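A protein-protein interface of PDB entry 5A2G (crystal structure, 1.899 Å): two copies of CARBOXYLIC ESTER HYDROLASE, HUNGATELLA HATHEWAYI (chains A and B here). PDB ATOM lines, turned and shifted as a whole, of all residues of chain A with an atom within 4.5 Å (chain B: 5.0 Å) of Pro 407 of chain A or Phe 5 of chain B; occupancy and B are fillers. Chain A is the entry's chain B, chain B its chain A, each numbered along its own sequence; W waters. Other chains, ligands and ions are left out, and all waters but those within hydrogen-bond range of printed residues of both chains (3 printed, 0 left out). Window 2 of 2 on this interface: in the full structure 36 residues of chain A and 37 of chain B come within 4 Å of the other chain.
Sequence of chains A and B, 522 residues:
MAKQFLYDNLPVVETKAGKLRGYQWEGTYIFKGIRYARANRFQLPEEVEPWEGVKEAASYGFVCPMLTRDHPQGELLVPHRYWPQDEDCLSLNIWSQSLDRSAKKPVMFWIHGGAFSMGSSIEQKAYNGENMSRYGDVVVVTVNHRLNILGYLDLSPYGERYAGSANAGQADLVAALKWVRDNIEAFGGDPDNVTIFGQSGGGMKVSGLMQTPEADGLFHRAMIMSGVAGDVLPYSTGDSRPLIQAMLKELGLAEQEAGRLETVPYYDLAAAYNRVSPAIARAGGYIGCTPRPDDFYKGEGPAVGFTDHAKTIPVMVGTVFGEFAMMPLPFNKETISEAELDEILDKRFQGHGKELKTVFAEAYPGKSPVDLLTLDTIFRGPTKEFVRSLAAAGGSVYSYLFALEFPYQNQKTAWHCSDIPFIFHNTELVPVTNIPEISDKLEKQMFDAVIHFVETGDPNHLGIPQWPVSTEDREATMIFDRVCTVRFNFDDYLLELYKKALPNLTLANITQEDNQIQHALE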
ATOM      1  N   LEU A  76     -29.677   0.324  26.608  1.00  0.00           N
ATOM      2  CA  LEU A  76     -28.604  -0.616  26.904  1.00  0.00           C
ATOM      3  C   LEU A  76     -27.785  -0.091  28.073  1.00  0.00           C
ATOM      4  O   LEU A  76     -27.329  -0.862  28.914  1.00  0.00           O
ATOM      5  CB  LEU A  76     -27.719  -0.849  25.688  1.00  0.00           C
ATOM      6  CG  LEU A  76     -28.352  -1.735  24.619  1.00  0.00           C
ATOM      7  CD1 LEU A  76     -27.393  -1.933  23.471  1.00  0.00           C
ATOM      8  CD2 LEU A  76     -28.782  -3.078  25.219  1.00  0.00           C
ATOM      9  N   GLU A 405     -14.676  -1.008  32.608  1.00  0.00           N
ATOM     10  CA  GLU A 405     -14.927  -0.732  31.199  1.00  0.00           C
ATOM     11  C   GLU A 405     -15.829  -1.824  30.626  1.00  0.00           C
ATOM     12  O   GLU A 405     -15.692  -2.990  30.994  1.00  0.00           O
ATOM     13  CB  GLU A 405     -13.609  -0.644  30.426  1.00  0.00           C
ATOM     14  CG  GLU A 405     -12.704   0.483  30.903  1.00  0.00           C
ATOM     15  CD  GLU A 405     -11.270   0.285  30.483  1.00  0.00           C
ATOM     16  OE1 GLU A 405     -10.510  -0.360  31.237  1.00  0.00           O
ATOM     17  OE2 GLU A 405     -10.901   0.770  29.397  1.00  0.00           O
ATOM     18  N   PHE A 406     -16.736  -1.442  29.726  1.00  0.00           N
ATOM     19  CA  PHE A 406     -17.850  -2.307  29.315  1.00  0.00           C
ATOM     20  C   PHE A 406     -17.785  -2.782  27.857  1.00  0.00           C
ATOM     21  O   PHE A 406     -17.229  -2.093  27.005  1.00  0.00           O
ATOM     22  CB  PHE A 406     -19.172  -1.572  29.559  1.00  0.00           C
ATOM     23  CG  PHE A 406     -19.532  -1.464  31.006  1.00  0.00           C
ATOM     24  CD1 PHE A 406     -19.048  -0.416  31.772  1.00  0.00           C
ATOM     25  CD2 PHE A 406     -20.327  -2.422  31.609  1.00  0.00           C
ATOM     26  CE1 PHE A 406     -19.364  -0.315  33.102  1.00  0.00           C
ATOM     27  CE2 PHE A 406     -20.646  -2.329  32.948  1.00  0.00           C
ATOM     28  CZ  PHE A 406     -20.161  -1.268  33.698  1.00  0.00           C
ATOM     29  N   PRO A 407     -18.361  -3.964  27.573  1.00  0.00           N
ATOM     30  CA  PRO A 407     -18.358  -4.581  26.239  1.00  0.00           C
ATOM     31  C   PRO A 407     -19.351  -3.916  25.302  1.00  0.00           C
ATOM     32  O   PRO A 407     -20.291  -4.551  24.821  1.00  0.00           O
ATOM     33  CB  PRO A 407     -18.767  -6.024  26.525  1.00  0.00           C
ATOM     34  CG  PRO A 407     -19.651  -5.906  27.724  1.00  0.00           C
ATOM     35  CD  PRO A 407     -19.027  -4.828  28.566  1.00  0.00           C
ATOM     36  N   TYR A 408     -19.116  -2.639  25.037  1.00  0.00           N
ATOM     37  CA  TYR A 408     -20.043  -1.802  24.304  1.00  0.00           C
ATOM     38  C   TYR A 408     -19.273  -0.595  23.788  1.00  0.00           C
ATOM     39  O   TYR A 408     -18.604   0.084  24.560  1.00  0.00           O
ATOM     40  CB  TYR A 408     -21.200  -1.392  25.217  1.00  0.00           C
ATOM     41  CG  TYR A 408     -22.260  -0.496  24.613  1.00  0.00           C
ATOM     42  CD1 TYR A 408     -23.254  -1.013  23.788  1.00  0.00           C
ATOM     43  CD2 TYR A 408     -22.295   0.859  24.906  1.00  0.00           C
ATOM     44  CE1 TYR A 408     -24.237  -0.198  23.252  1.00  0.00           C
ATOM     45  CE2 TYR A 408     -23.272   1.683  24.372  1.00  0.00           C
ATOM     46  CZ  TYR A 408     -24.241   1.147  23.548  1.00  0.00           C
ATOM     47  OH  TYR A 408     -25.215   1.968  23.022  1.00  0.00           O
ATOM     48  N   PRO A 431     -28.223  -6.199  30.583  1.00  0.00           N
ATOM     49  CA  PRO A 431     -27.432  -7.025  29.660  1.00  0.00           C
ATOM     50  C   PRO A 431     -26.006  -6.523  29.401  1.00  0.00           C
ATOM     51  O   PRO A 431     -25.088  -7.338  29.434  1.00  0.00           O
ATOM     52  CB  PRO A 431     -28.271  -7.000  28.383  1.00  0.00           C
ATOM     53  CG  PRO A 431     -29.694  -6.906  28.901  1.00  0.00           C
ATOM     54  CD  PRO A 431     -29.602  -5.987  30.097  1.00  0.00           C
ATOM     55  N   VAL A 432     -25.823  -5.221  29.193  1.00  0.00           N
ATOM     56  CA  VAL A 432     -24.514  -4.660  28.842  1.00  0.00           C
ATOM     57  C   VAL A 432     -23.451  -4.867  29.929  1.00  0.00           C
ATOM     58  O   VAL A 432     -22.254  -4.884  29.639  1.00  0.00           O
ATOM     59  CB  VAL A 432     -24.622  -3.150  28.540  1.00  0.00           C
ATOM     60  CG1 VAL A 432     -24.804  -2.355  29.826  1.00  0.00           C
ATOM     61  CG2 VAL A 432     -23.396  -2.661  27.781  1.00  0.00           C
ATOM     62  N   ASN A 434     -22.835  -7.527  31.496  1.00  0.00           N
ATOM     63  CA  ASN A 434     -22.367  -8.906  31.557  1.00  0.00           C
ATOM     64  C   ASN A 434     -21.069  -9.106  30.788  1.00  0.00           C
ATOM     65  O   ASN A 434     -21.016  -8.941  29.564  1.00  0.00           O
ATOM     66  CB  ASN A 434     -23.445  -9.858  31.056  1.00  0.00           C
ATOM     67  CG  ASN A 434     -24.597  -9.965  32.026  1.00  0.00           C
ATOM     68  OD1 ASN A 434     -24.677 -10.911  32.811  1.00  0.00           O
ATOM     69  ND2 ASN A 434     -25.472  -8.960  32.017  1.00  0.00           N
ATOM     70  N   ILE A 435     -20.018  -9.435  31.539  1.00  0.00           N
ATOM     71  CA  ILE A 435     -18.702  -9.697  30.974  1.00  0.00           C
ATOM     72  C   ILE A 435     -18.174 -11.031  31.483  1.00  0.00           C
ATOM     73  O   ILE A 435     -18.026 -11.212  32.692  1.00  0.00           O
ATOM     74  CB  ILE A 435     -17.691  -8.601  31.335  1.00  0.00           C
ATOM     75  CG1 ILE A 435     -18.360  -7.223  31.336  1.00  0.00           C
ATOM     76  CG2 ILE A 435     -16.496  -8.657  30.389  1.00  0.00           C
ATOM     77  CD1 ILE A 435     -17.528  -6.140  31.982  1.00  0.00           C
ATOM     78  N   LYS B   3     -24.377 -14.085  32.142  1.00  0.00           N
ATOM     79  CA  LYS B   3     -25.279 -14.232  31.004  1.00  0.00           C
ATOM     80  C   LYS B   3     -24.593 -13.753  29.725  1.00  0.00           C
ATOM     81  O   LYS B   3     -23.764 -12.842  29.766  1.00  0.00           O
ATOM     82  CB  LYS B   3     -26.569 -13.442  31.218  1.00  0.00           C
ATOM     83  CG  LYS B   3     -27.343 -13.764  32.483  1.00  0.00           C
ATOM     84  CD  LYS B   3     -28.048 -15.098  32.370  1.00  0.00           C
ATOM     85  CE  LYS B   3     -29.438 -15.067  33.013  1.00  0.00           C
ATOM     86  NZ  LYS B   3     -29.396 -14.771  34.472  1.00  0.00           N
ATOM     87  N   GLN B   4     -24.949 -14.356  28.595  1.00  0.00           N
ATOM     88  CA  GLN B   4     -24.331 -14.018  27.313  1.00  0.00           C
ATOM     89  C   GLN B   4     -24.829 -12.674  26.777  1.00  0.00           C
ATOM     90  O   GLN B   4     -26.030 -12.469  26.635  1.00  0.00           O
ATOM     91  CB  GLN B   4     -24.599 -15.127  26.287  1.00  0.00           C
ATOM     92  CG  GLN B   4     -23.722 -15.070  25.034  1.00  0.00           C
ATOM     93  CD  GLN B   4     -24.363 -14.328  23.865  1.00  0.00           C
ATOM     94  OE1 GLN B   4     -25.558 -14.026  23.874  1.00  0.00           O
ATOM     95  NE2 GLN B   4     -23.560 -14.036  22.846  1.00  0.00           N
ATOM     96  N   PHE B   5     -23.903 -11.762  26.490  1.00  0.00           N
ATOM     97  CA  PHE B   5     -24.246 -10.493  25.846  1.00  0.00           C
ATOM     98  C   PHE B   5     -23.206 -10.100  24.804  1.00  0.00           C
ATOM     99  O   PHE B   5     -22.007 -10.136  25.068  1.00  0.00           O
ATOM    100  CB  PHE B   5     -24.381  -9.355  26.865  1.00  0.00           C
ATOM    101  CG  PHE B   5     -24.478  -7.980  26.229  1.00  0.00           C
ATOM    102  CD1 PHE B   5     -25.700  -7.485  25.796  1.00  0.00           C
ATOM    103  CD2 PHE B   5     -23.349  -7.194  26.054  1.00  0.00           C
ATOM    104  CE1 PHE B   5     -25.794  -6.234  25.208  1.00  0.00           C
ATOM    105  CE2 PHE B   5     -23.436  -5.941  25.465  1.00  0.00           C
ATOM    106  CZ  PHE B   5     -24.660  -5.456  25.045  1.00  0.00           C
ATOM    107  N   LEU B   6     -23.676  -9.702  23.630  1.00  0.00           N
ATOM    108  CA  LEU B   6     -22.788  -9.206  22.587  1.00  0.00           C
ATOM    109  C   LEU B   6     -23.393  -7.984  21.928  1.00  0.00           C
ATOM    110  O   LEU B   6     -24.619  -7.868  21.832  1.00  0.00           O
ATOM    111  CB  LEU B   6     -22.514 -10.286  21.539  1.00  0.00           C
ATOM    112  CG  LEU B   6     -21.503 -11.372  21.906  1.00  0.00           C
ATOM    113  CD1 LEU B   6     -21.303 -12.320  20.728  1.00  0.00           C
ATOM    114  CD2 LEU B   6     -20.179 -10.761  22.349  1.00  0.00           C
ATOM    115  N   TYR B   7     -22.529  -7.076  21.481  1.00  0.00           N
ATOM    116  CA  TYR B   7     -22.963  -5.864  20.796  1.00  0.00           C
ATOM    117  C   TYR B   7     -22.033  -5.496  19.636  1.00  0.00           C
ATOM    118  O   TYR B   7     -22.452  -5.474  18.475  1.00  0.00           O
ATOM    119  CB  TYR B   7     -23.052  -4.698  21.780  1.00  0.00           C
ATOM    120  CG  TYR B   7     -23.516  -3.411  21.142  1.00  0.00           C
ATOM    121  CD1 TYR B   7     -24.862  -3.144  20.986  1.00  0.00           C
ATOM    122  CD2 TYR B   7     -22.605  -2.470  20.681  1.00  0.00           C
ATOM    123  CE1 TYR B   7     -25.298  -1.970  20.398  1.00  0.00           C
ATOM    124  CE2 TYR B   7     -23.030  -1.292  20.083  1.00  0.00           C
ATOM    125  CZ  TYR B   7     -24.379  -1.051  19.948  1.00  0.00           C
ATOM    126  OH  TYR B   7     -24.824   0.111  19.370  1.00  0.00           O
ATOM    127  N   ASP B   8     -20.770  -5.227  19.957  1.00  0.00           N
ATOM    128  CA  ASP B   8     -19.826  -4.654  18.995  1.00  0.00           C
ATOM    129  C   ASP B   8     -19.601  -5.443  17.698  1.00  0.00           C
ATOM    130  O   ASP B   8     -19.709  -4.889  16.604  1.00  0.00           O
ATOM    131  CB  ASP B   8     -18.479  -4.438  19.675  1.00  0.00           C
ATOM    132  CG  ASP B   8     -18.489  -3.249  20.611  1.00  0.00           C
ATOM    133  OD1 ASP B   8     -19.371  -2.377  20.469  1.00  0.00           O
ATOM    134  OD2 ASP B   8     -17.607  -3.186  21.487  1.00  0.00           O
ATOM    135  N   TYR B  23     -28.711  -5.941  19.702  1.00  0.00           N
ATOM    136  CA  TYR B  23     -27.794  -6.680  20.553  1.00  0.00           C
ATOM    137  C   TYR B  23     -28.139  -8.154  20.554  1.00  0.00           C
ATOM    138  O   TYR B  23     -29.107  -8.583  19.923  1.00  0.00           O
ATOM    139  CB  TYR B  23     -27.771  -6.118  21.989  1.00  0.00           C
ATOM    140  CG  TYR B  23     -29.092  -6.087  22.740  1.00  0.00           C
ATOM    141  CD1 TYR B  23     -30.086  -5.180  22.399  1.00  0.00           C
ATOM    142  CD2 TYR B  23     -29.323  -6.937  23.816  1.00  0.00           C
ATOM    143  CE1 TYR B  23     -31.280  -5.136  23.087  1.00  0.00           C
ATOM    144  CE2 TYR B  23     -30.510  -6.896  24.518  1.00  0.00           C
ATOM    145  CZ  TYR B  23     -31.486  -5.997  24.142  1.00  0.00           C
ATOM    146  OH  TYR B  23     -32.668  -5.948  24.829  1.00  0.00           O
ATOM    147  N   GLN B  24     -27.303  -8.932  21.225  1.00  0.00           N
ATOM    148  CA  GLN B  24     -27.555 -10.348  21.385  1.00  0.00           C
ATOM    149  C   GLN B  24     -27.567 -10.657  22.867  1.00  0.00           C
ATOM    150  O   GLN B  24     -26.740 -10.152  23.624  1.00  0.00           O
ATOM    151  CB  GLN B  24     -26.504 -11.187  20.654  1.00  0.00           C
ATOM    152  CG  GLN B  24     -26.872 -12.660  20.549  1.00  0.00           C
ATOM    153  CD  GLN B  24     -25.856 -13.468  19.765  1.00  0.00           C
ATOM    154  OE1 GLN B  24     -24.663 -13.155  19.760  1.00  0.00           O
ATOM    155  NE2 GLN B  24     -26.329 -14.513  19.088  1.00  0.00           N
ATOM    156  N   TRP B  25     -28.520 -11.482  23.278  1.00  0.00           N
ATOM    157  CA  TRP B  25     -28.698 -11.806  24.682  1.00  0.00           C
ATOM    158  C   TRP B  25     -29.092 -13.268  24.785  1.00  0.00           C
ATOM    159  O   TRP B  25     -30.082 -13.699  24.177  1.00  0.00           O
ATOM    160  CB  TRP B  25     -29.750 -10.888  25.309  1.00  0.00           C
ATOM    161  CG  TRP B  25     -30.148 -11.206  26.737  1.00  0.00           C
ATOM    162  CD1 TRP B  25     -31.336 -11.735  27.153  1.00  0.00           C
ATOM    163  CD2 TRP B  25     -29.373 -10.982  27.928  1.00  0.00           C
ATOM    164  NE1 TRP B  25     -31.349 -11.860  28.524  1.00  0.00           N
ATOM    165  CE2 TRP B  25     -30.155 -11.410  29.023  1.00  0.00           C
ATOM    166  CE3 TRP B  25     -28.094 -10.476  28.171  1.00  0.00           C
ATOM    167  CZ2 TRP B  25     -29.700 -11.344  30.341  1.00  0.00           C
ATOM    168  CZ3 TRP B  25     -27.641 -10.410  29.492  1.00  0.00           C
ATOM    169  CH2 TRP B  25     -28.450 -10.828  30.555  1.00  0.00           C
HETATM  170  O   HOH W   1     -20.183  -6.207  22.731  1.00  0.00           O
HETATM  171  O   HOH W   2     -16.233  -3.417  23.688  1.00  0.00           O
HETATM  172  O   HOH W   3     -20.122  -9.602  26.979  1.00  0.00           O
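The backbone NH (N) of Lys 3 of chain B lies within hydrogen-bond range of the side-chain amide oxygen (OD1) of Asn 434 of chain A, at 3.3 Å.
The backbone carbonyl oxygen (O) of Pro 431 of chain A sits at hydrogen-bond distance from the side-chain amide nitrogen (ND2) of Asn 434 of chain A (3.1 Å).
Leu 76 of chain A touches Tyr 7 of chain B (CD1 to CE1, 3.7 Å).
CD2 of Leu 76 of chain A touches CD1 of Tyr 23 of chain B, 3.8 Å away.
Pro 407 of chain A touches Phe 5 of chain B (O to CE2, 3.5 Å).
Tyr 7 of chain B touches Tyr 408 of chain A.
Asp 8 of chain B touches Tyr 408 of chain A (OD1 to C, 3.8 Å).
Phe 5 of chain B touches Pro 431 of chain A (CG to O, 3.3 Å).
Trp 25 of chain B touches Pro 431 of chain A.
Val 432 of chain A touches Phe 5 of chain B.
Asn 434 of chain A touches Trp 25 of chain B.
Of chain B, only Phe 5 (3.5 Å) comes within 4 Å of Pro 407 of chain A.
Of chain A, only Pro 407, Pro 431 and Val 432 come within 4 Å of Phe 5 of chain B.
Printed residues of chain B within 4 Å of Val 432 of chain A: Phe 5.
Of the printed residues of chain A, Trp 25 of chain B touches Pro 431 (3.4 Å) and Asn 434 (3.6 Å).
Of the printed residues of chain A, Tyr 7 of chain B touches Leu 76 (3.7 Å) and Tyr 408 (3.4 Å).
The nearest printed residue of chain A that does not touch Phe 5 of chain B is Asn 434 of chain A (4.3 Å).
Of the 9 printed residues of chain B, 6 touch a printed residue of chain A.
Hydrophobic or aromatic side chains of chain B within 4 Å of the printed part of chain A: Phe 5, Tyr 7, Tyr 23 and Trp 25.
Among the printed residues, 10 pairs touch across the chains.
Among the printed residues, no Asp or Glu carboxylate lies within 4 Å of a Lys or Arg side-chain nitrogen of the other chain.
No position is printed for both chains.
Water W2 bridges the side-chain carboxylate (OD2) of Asp 8 of chain B and the backbone NH (N) of Tyr 408 of chain A.
Water W1 lies within hydrogen-bond range of O of Pro 407 of chain A (2.7 Å), N of Tyr 7 of chain B (2.8 Å) and N of Asp 8 of chain B (3.0 Å).
Water W3 bridges O of Phe 5 of chain B and O of Asn 434 of chain A.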
